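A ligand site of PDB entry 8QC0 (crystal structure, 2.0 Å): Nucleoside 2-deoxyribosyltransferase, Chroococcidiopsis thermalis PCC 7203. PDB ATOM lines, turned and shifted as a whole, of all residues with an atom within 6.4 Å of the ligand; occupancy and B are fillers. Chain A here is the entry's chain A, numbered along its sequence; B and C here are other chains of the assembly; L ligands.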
ATOM      1  N   TYR A   7      -3.443  -7.751 -16.133  1.00  0.00           N
ATOM      2  CA  TYR A   7      -3.895  -9.107 -15.875  1.00  0.00           C
ATOM      3  C   TYR A   7      -2.674 -10.018 -15.736  1.00  0.00           C
ATOM      4  O   TYR A   7      -1.870 -10.120 -16.670  1.00  0.00           O
ATOM      5  CB  TYR A   7      -4.798  -9.583 -16.996  1.00  0.00           C
ATOM      6  CG  TYR A   7      -5.420 -10.938 -16.797  1.00  0.00           C
ATOM      7  CD1 TYR A   7      -6.611 -11.089 -16.082  1.00  0.00           C
ATOM      8  CD2 TYR A   7      -4.827 -12.087 -17.329  1.00  0.00           C
ATOM      9  CE1 TYR A   7      -7.199 -12.337 -15.912  1.00  0.00           C
ATOM     10  CE2 TYR A   7      -5.414 -13.345 -17.155  1.00  0.00           C
ATOM     11  CZ  TYR A   7      -6.600 -13.451 -16.443  1.00  0.00           C
ATOM     12  OH  TYR A   7      -7.193 -14.676 -16.268  1.00  0.00           O
ATOM     13  N   ALA A   9      -1.390 -13.375 -15.745  1.00  0.00           N
ATOM     14  CA  ALA A   9      -1.652 -14.751 -16.127  1.00  0.00           C
ATOM     15  C   ALA A   9      -0.471 -15.638 -15.731  1.00  0.00           C
ATOM     16  O   ALA A   9       0.690 -15.271 -15.955  1.00  0.00           O
ATOM     17  CB  ALA A   9      -1.899 -14.848 -17.631  1.00  0.00           C
ATOM     18  N   SER A  10      -0.769 -16.801 -15.136  1.00  0.00           N
ATOM     19  CA  SER A  10       0.273 -17.681 -14.624  1.00  0.00           C
ATOM     20  C   SER A  10      -0.343 -19.039 -14.331  1.00  0.00           C
ATOM     21  O   SER A  10      -1.557 -19.127 -14.128  1.00  0.00           O
ATOM     22  CB  SER A  10       0.907 -17.122 -13.345  1.00  0.00           C
ATOM     23  OG  SER A  10       0.168 -17.576 -12.211  1.00  0.00           O
ATOM     24  N   PRO A  11       0.462 -20.100 -14.287  1.00  0.00           N
ATOM     25  CA  PRO A  11       0.005 -21.385 -13.759  1.00  0.00           C
ATOM     26  C   PRO A  11       0.243 -21.564 -12.269  1.00  0.00           C
ATOM     27  O   PRO A  11      -0.034 -22.639 -11.741  1.00  0.00           O
ATOM     28  CB  PRO A  11       0.863 -22.394 -14.550  1.00  0.00           C
ATOM     29  CG  PRO A  11       2.173 -21.687 -14.716  1.00  0.00           C
ATOM     30  CD  PRO A  11       1.868 -20.169 -14.726  1.00  0.00           C
ATOM     31  N   PHE A  14      -2.012 -23.335  -9.562  1.00  0.00           N
ATOM     32  CA  PHE A  14      -2.349 -24.759  -9.549  1.00  0.00           C
ATOM     33  C   PHE A  14      -1.627 -25.527  -8.447  1.00  0.00           C
ATOM     34  O   PHE A  14      -2.111 -26.571  -7.992  1.00  0.00           O
ATOM     35  CB  PHE A  14      -2.054 -25.392 -10.916  1.00  0.00           C
ATOM     36  CG  PHE A  14      -2.938 -24.886 -12.018  1.00  0.00           C
ATOM     37  CD1 PHE A  14      -4.316 -24.976 -11.910  1.00  0.00           C
ATOM     38  CD2 PHE A  14      -2.398 -24.268 -13.127  1.00  0.00           C
ATOM     39  CE1 PHE A  14      -5.146 -24.496 -12.922  1.00  0.00           C
ATOM     40  CE2 PHE A  14      -3.229 -23.779 -14.144  1.00  0.00           C
ATOM     41  CZ  PHE A  14      -4.597 -23.889 -14.035  1.00  0.00           C
ATOM     42  N   PRO A  40      -5.940 -13.743 -11.555  1.00  0.00           N
ATOM     43  CA  PRO A  40      -7.176 -14.543 -11.672  1.00  0.00           C
ATOM     44  C   PRO A  40      -7.395 -15.554 -10.562  1.00  0.00           C
ATOM     45  O   PRO A  40      -8.549 -15.814 -10.222  1.00  0.00           O
ATOM     46  CB  PRO A  40      -7.013 -15.270 -13.026  1.00  0.00           C
ATOM     47  CG  PRO A  40      -5.538 -15.215 -13.346  1.00  0.00           C
ATOM     48  CD  PRO A  40      -5.027 -13.946 -12.704  1.00  0.00           C
ATOM     49  N   PHE A  41      -6.350 -16.150  -9.987  1.00  0.00           N
ATOM     50  CA  PHE A  41      -6.602 -17.124  -8.932  1.00  0.00           C
ATOM     51  C   PHE A  41      -7.161 -16.439  -7.687  1.00  0.00           C
ATOM     52  O   PHE A  41      -8.116 -16.918  -7.086  1.00  0.00           O
ATOM     53  CB  PHE A  41      -5.347 -17.935  -8.606  1.00  0.00           C
ATOM     54  CG  PHE A  41      -4.989 -18.919  -9.683  1.00  0.00           C
ATOM     55  CD1 PHE A  41      -5.724 -20.079  -9.824  1.00  0.00           C
ATOM     56  CD2 PHE A  41      -3.982 -18.641 -10.596  1.00  0.00           C
ATOM     57  CE1 PHE A  41      -5.414 -20.995 -10.847  1.00  0.00           C
ATOM     58  CE2 PHE A  41      -3.665 -19.552 -11.613  1.00  0.00           C
ATOM     59  CZ  PHE A  41      -4.400 -20.707 -11.741  1.00  0.00           C
ATOM     60  N   ASN A  44     -10.624 -15.448  -8.345  1.00  0.00           N
ATOM     61  CA  ASN A  44     -11.457 -16.662  -8.504  1.00  0.00           C
ATOM     62  C   ASN A  44     -12.216 -16.684  -9.838  1.00  0.00           C
ATOM     63  O   ASN A  44     -11.633 -16.850 -10.928  1.00  0.00           O
ATOM     64  CB  ASN A  44     -12.432 -16.812  -7.337  1.00  0.00           C
ATOM     65  CG  ASN A  44     -11.787 -17.428  -6.126  1.00  0.00           C
ATOM     66  OD1 ASN A  44     -11.559 -18.637  -6.081  1.00  0.00           O
ATOM     67  ND2 ASN A  44     -11.484 -16.608  -5.121  1.00  0.00           N
ATOM     68  N   VAL A  58     -16.195 -19.359 -14.584  1.00  0.00           N
ATOM     69  CA  VAL A  58     -14.814 -18.916 -14.396  1.00  0.00           C
ATOM     70  C   VAL A  58     -14.195 -18.537 -15.740  1.00  0.00           C
ATOM     71  O   VAL A  58     -13.522 -17.502 -15.855  1.00  0.00           O
ATOM     72  CB  VAL A  58     -13.986 -19.992 -13.675  1.00  0.00           C
ATOM     73  CG1 VAL A  58     -12.483 -19.716 -13.836  1.00  0.00           C
ATOM     74  CG2 VAL A  58     -14.391 -20.011 -12.210  1.00  0.00           C
ATOM     75  N   ALA A  59     -14.444 -19.347 -16.778  1.00  0.00           N
ATOM     76  CA  ALA A  59     -13.901 -19.007 -18.092  1.00  0.00           C
ATOM     77  C   ALA A  59     -14.416 -17.658 -18.558  1.00  0.00           C
ATOM     78  O   ALA A  59     -13.658 -16.852 -19.119  1.00  0.00           O
ATOM     79  CB  ALA A  59     -14.247 -20.106 -19.101  1.00  0.00           C
ATOM     80  N   ASP A  62     -12.775 -14.700 -16.360  1.00  0.00           N
ATOM     81  CA  ASP A  62     -11.410 -14.343 -16.720  1.00  0.00           C
ATOM     82  C   ASP A  62     -11.343 -13.725 -18.112  1.00  0.00           C
ATOM     83  O   ASP A  62     -10.561 -12.798 -18.355  1.00  0.00           O
ATOM     84  CB  ASP A  62     -10.508 -15.574 -16.631  1.00  0.00           C
ATOM     85  CG  ASP A  62     -10.321 -16.045 -15.195  1.00  0.00           C
ATOM     86  OD1 ASP A  62     -10.597 -15.253 -14.271  1.00  0.00           O
ATOM     87  OD2 ASP A  62      -9.911 -17.208 -14.987  1.00  0.00           O
ATOM     88  N   LEU A  63     -12.179 -14.221 -19.031  1.00  0.00           N
ATOM     89  CA  LEU A  63     -12.291 -13.592 -20.348  1.00  0.00           C
ATOM     90  C   LEU A  63     -12.679 -12.121 -20.217  1.00  0.00           C
ATOM     91  O   LEU A  63     -12.085 -11.249 -20.873  1.00  0.00           O
ATOM     92  CB  LEU A  63     -13.330 -14.339 -21.197  1.00  0.00           C
ATOM     93  CG  LEU A  63     -13.671 -13.663 -22.540  1.00  0.00           C
ATOM     94  CD1 LEU A  63     -12.396 -13.347 -23.332  1.00  0.00           C
ATOM     95  CD2 LEU A  63     -14.621 -14.519 -23.378  1.00  0.00           C
ATOM     96  N   ASP A  82       2.070 -22.680 -20.016  1.00  0.00           N
ATOM     97  CA  ASP A  82       0.775 -23.235 -19.662  1.00  0.00           C
ATOM     98  C   ASP A  82      -0.277 -22.882 -20.718  1.00  0.00           C
ATOM     99  O   ASP A  82      -0.312 -21.762 -21.228  1.00  0.00           O
ATOM    100  CB  ASP A  82       0.382 -22.715 -18.272  1.00  0.00           C
ATOM    101  CG  ASP A  82      -1.050 -23.059 -17.896  1.00  0.00           C
ATOM    102  OD1 ASP A  82      -1.963 -22.310 -18.295  1.00  0.00           O
ATOM    103  OD2 ASP A  82      -1.263 -24.078 -17.198  1.00  0.00           O
ATOM    104  N   GLU A  83      -1.151 -23.848 -21.054  1.00  0.00           N
ATOM    105  CA  GLU A  83      -2.076 -23.630 -22.157  1.00  0.00           C
ATOM    106  C   GLU A  83      -3.133 -22.566 -21.825  1.00  0.00           C
ATOM    107  O   GLU A  83      -3.611 -21.869 -22.735  1.00  0.00           O
ATOM    108  CB  GLU A  83      -2.734 -24.955 -22.564  1.00  0.00           C
ATOM    109  CG  GLU A  83      -3.741 -25.520 -21.566  1.00  0.00           C
ATOM    110  CD  GLU A  83      -3.080 -26.498 -20.631  1.00  0.00           C
ATOM    111  OE1 GLU A  83      -1.904 -26.260 -20.238  1.00  0.00           O
ATOM    112  OE2 GLU A  83      -3.706 -27.517 -20.299  1.00  0.00           O
ATOM    113  N   GLY A  84      -3.501 -22.406 -20.558  1.00  0.00           N
ATOM    114  CA  GLY A  84      -4.460 -21.361 -20.223  1.00  0.00           C
ATOM    115  C   GLY A  84      -3.854 -19.982 -20.356  1.00  0.00           C
ATOM    116  O   GLY A  84      -4.485 -19.056 -20.860  1.00  0.00           O
ATOM    117  N   VAL A  85      -2.614 -19.823 -19.896  1.00  0.00           N
ATOM    118  CA  VAL A  85      -1.898 -18.575 -20.109  1.00  0.00           C
ATOM    119  C   VAL A  85      -1.802 -18.256 -21.588  1.00  0.00           C
ATOM    120  O   VAL A  85      -1.962 -17.101 -22.001  1.00  0.00           O
ATOM    121  CB  VAL A  85      -0.506 -18.636 -19.467  1.00  0.00           C
ATOM    122  CG1 VAL A  85       0.307 -17.379 -19.842  1.00  0.00           C
ATOM    123  CG2 VAL A  85      -0.637 -18.809 -17.967  1.00  0.00           C
ATOM    124  N   GLU A  88      -5.043 -16.941 -22.932  1.00  0.00           N
ATOM    125  CA  GLU A  88      -5.201 -15.569 -22.460  1.00  0.00           C
ATOM    126  C   GLU A  88      -4.233 -14.630 -23.164  1.00  0.00           C
ATOM    127  O   GLU A  88      -4.581 -13.489 -23.506  1.00  0.00           O
ATOM    128  CB  GLU A  88      -5.022 -15.528 -20.942  1.00  0.00           C
ATOM    129  CG  GLU A  88      -6.278 -15.956 -20.110  1.00  0.00           C
ATOM    130  CD  GLU A  88      -5.919 -16.494 -18.717  1.00  0.00           C
ATOM    131  OE1 GLU A  88      -4.741 -16.370 -18.330  1.00  0.00           O
ATOM    132  OE2 GLU A  88      -6.814 -16.979 -17.982  1.00  0.00           O
ATOM    133  N   ASP B 111      -7.869 -28.745 -15.577  1.00  0.00           N
ATOM    134  CA  ASP B 111      -7.933 -28.123 -14.260  1.00  0.00           C
ATOM    135  C   ASP B 111      -9.351 -28.102 -13.694  1.00  0.00           C
ATOM    136  O   ASP B 111      -9.632 -27.294 -12.808  1.00  0.00           O
ATOM    137  CB  ASP B 111      -7.396 -26.697 -14.300  1.00  0.00           C
ATOM    138  CG  ASP B 111      -8.229 -25.782 -15.182  1.00  0.00           C
ATOM    139  OD1 ASP B 111      -9.039 -26.293 -15.971  1.00  0.00           O
ATOM    140  OD2 ASP B 111      -8.097 -24.546 -15.052  1.00  0.00           O
ATOM    141  N   ASN B 118      -8.175 -27.737 -19.907  1.00  0.00           N
ATOM    142  CA  ASN B 118      -8.226 -26.435 -19.241  1.00  0.00           C
ATOM    143  C   ASN B 118      -9.461 -25.661 -19.713  1.00  0.00           C
ATOM    144  O   ASN B 118      -9.701 -25.527 -20.923  1.00  0.00           O
ATOM    145  CB  ASN B 118      -6.937 -25.667 -19.540  1.00  0.00           C
ATOM    146  CG  ASN B 118      -6.811 -24.380 -18.747  1.00  0.00           C
ATOM    147  OD1 ASN B 118      -7.670 -23.494 -18.857  1.00  0.00           O
ATOM    148  ND2 ASN B 118      -5.744 -24.237 -17.971  1.00  0.00           N
ATOM    149  N   LEU B 119     -10.249 -25.174 -18.751  1.00  0.00           N
ATOM    150  CA  LEU B 119     -11.558 -24.588 -19.076  1.00  0.00           C
ATOM    151  C   LEU B 119     -11.454 -23.388 -19.992  1.00  0.00           C
ATOM    152  O   LEU B 119     -12.450 -23.004 -20.622  1.00  0.00           O
ATOM    153  CB  LEU B 119     -12.288 -24.183 -17.793  1.00  0.00           C
ATOM    154  CG  LEU B 119     -11.501 -23.328 -16.790  1.00  0.00           C
ATOM    155  CD1 LEU B 119     -11.658 -21.844 -17.088  1.00  0.00           C
ATOM    156  CD2 LEU B 119     -11.918 -23.641 -15.353  1.00  0.00           C
ATOM    157  N   MET B 120     -10.287 -22.772 -20.084  1.00  0.00           N
ATOM    158  CA  MET B 120     -10.147 -21.577 -20.905  1.00  0.00           C
ATOM    159  C   MET B 120     -10.250 -21.869 -22.398  1.00  0.00           C
ATOM    160  O   MET B 120     -10.609 -20.972 -23.168  1.00  0.00           O
ATOM    161  CB  MET B 120      -8.818 -20.909 -20.553  1.00  0.00           C
ATOM    162  CG  MET B 120      -8.881 -19.404 -20.443  1.00  0.00           C
ATOM    163  SD  MET B 120     -10.262 -18.686 -19.496  1.00  0.00           S
ATOM    164  CE  MET B 120      -9.915 -16.976 -19.884  1.00  0.00           C
ATOM    165  N   ARG C 107      -4.121 -30.053 -10.916  1.00  0.00           N
ATOM    166  CA  ARG C 107      -4.467 -30.491 -12.254  1.00  0.00           C
ATOM    167  C   ARG C 107      -4.205 -31.985 -12.394  1.00  0.00           C
ATOM    168  O   ARG C 107      -3.362 -32.554 -11.697  1.00  0.00           O
ATOM    169  CB  ARG C 107      -3.668 -29.709 -13.303  1.00  0.00           C
ATOM    170  CG  ARG C 107      -4.042 -28.240 -13.417  1.00  0.00           C
ATOM    171  CD  ARG C 107      -3.049 -27.507 -14.302  1.00  0.00           C
ATOM    172  NE  ARG C 107      -1.691 -27.645 -13.767  1.00  0.00           N
ATOM    173  CZ  ARG C 107      -0.608 -27.104 -14.321  1.00  0.00           C
ATOM    174  NH1 ARG C 107      -0.689 -26.396 -15.448  1.00  0.00           N
ATOM    175  NH2 ARG C 107       0.571 -27.272 -13.732  1.00  0.00           N
HETATM  176  O1  LIG L   1      -4.159 -21.255 -16.615  1.00  0.00           O
HETATM  177  C1  LIG L   1      -4.468 -20.485 -15.491  1.00  0.00           C
HETATM  178  C2  LIG L   1      -5.504 -19.418 -15.859  1.00  0.00           C
HETATM  179  O2  LIG L   1      -5.259 -18.978 -17.063  1.00  0.00           O
HETATM  180  C3  LIG L   1      -6.953 -20.063 -15.963  1.00  0.00           C
HETATM  181  O3  LIG L   1      -7.740 -19.770 -14.933  1.00  0.00           O
HETATM  182  C4  LIG L   1      -7.506 -19.456 -17.221  1.00  0.00           C
HETATM  183  O4  LIG L   1      -8.814 -18.894 -16.906  1.00  0.00           O
HETATM  184  C5  LIG L   1      -6.652 -18.374 -17.636  1.00  0.00           C
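The side-chain carboxylate (OE2) of Glu 88 is bonded to a carbon (C5) of the ligand (1.4 Å). The side-chain carboxylate (OD2) of Asp 62 lies within hydrogen-bond range of an oxygen (O4) of the ligand (2.8 Å). OD1 of Asp 82 lies within hydrogen-bond range of O1 of the ligand (3.0 Å). The side-chain sulfur (SD) of Met 120 of chain B lies within hydrogen-bond range of an oxygen (O4) of the ligand, 3.0 Å away.
The side-chain carboxylate (OE2) of Glu 88 sits at hydrogen-bond distance from the side-chain hydroxyl (OH) of Tyr 7 (2.9 Å). The backbone NH (N) of Gly 84 lies within hydrogen-bond range of the side-chain carboxylate (OD1) of Asp 82. The backbone NH (N) of Val 85 is in hydrogen-bond range of the side-chain carboxylate (OD1) of Asp 82, 3.0 Å away. The guanidinium group of Arg 107 of chain C is in salt-bridge range of the side-chain carboxylate of Asp 82 (3.0 Å). N of Met 120 of chain B is in hydrogen-bond range of OD1 of Asn 118 of chain B (3.0 Å).
OH of Tyr 7 touches C5 of the ligand, at 3.98 Å. O of Ser 10 touches C1 of the ligand (3.5 Å). CE2 of Phe 14 touches O1 of the ligand, 3.7 Å away. Phe 41 touches the ligand (CZ to C1, 3.8 Å). Gly 84 touches the ligand (CA to O1, 3.6 Å). Val 85 touches the ligand (N to O1, 3.9 Å). ND2 of Asn 118 of chain B touches O1 of the ligand, 3.6 Å away. 11 residues have an atom within 4 Å of the ligand: Tyr 7, Ser 10, Phe 14, Phe 41, Asp 62, Asp 82, Gly 84, Val 85, Glu 88, Asn 118 of chain B and Met 120 of chain B.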
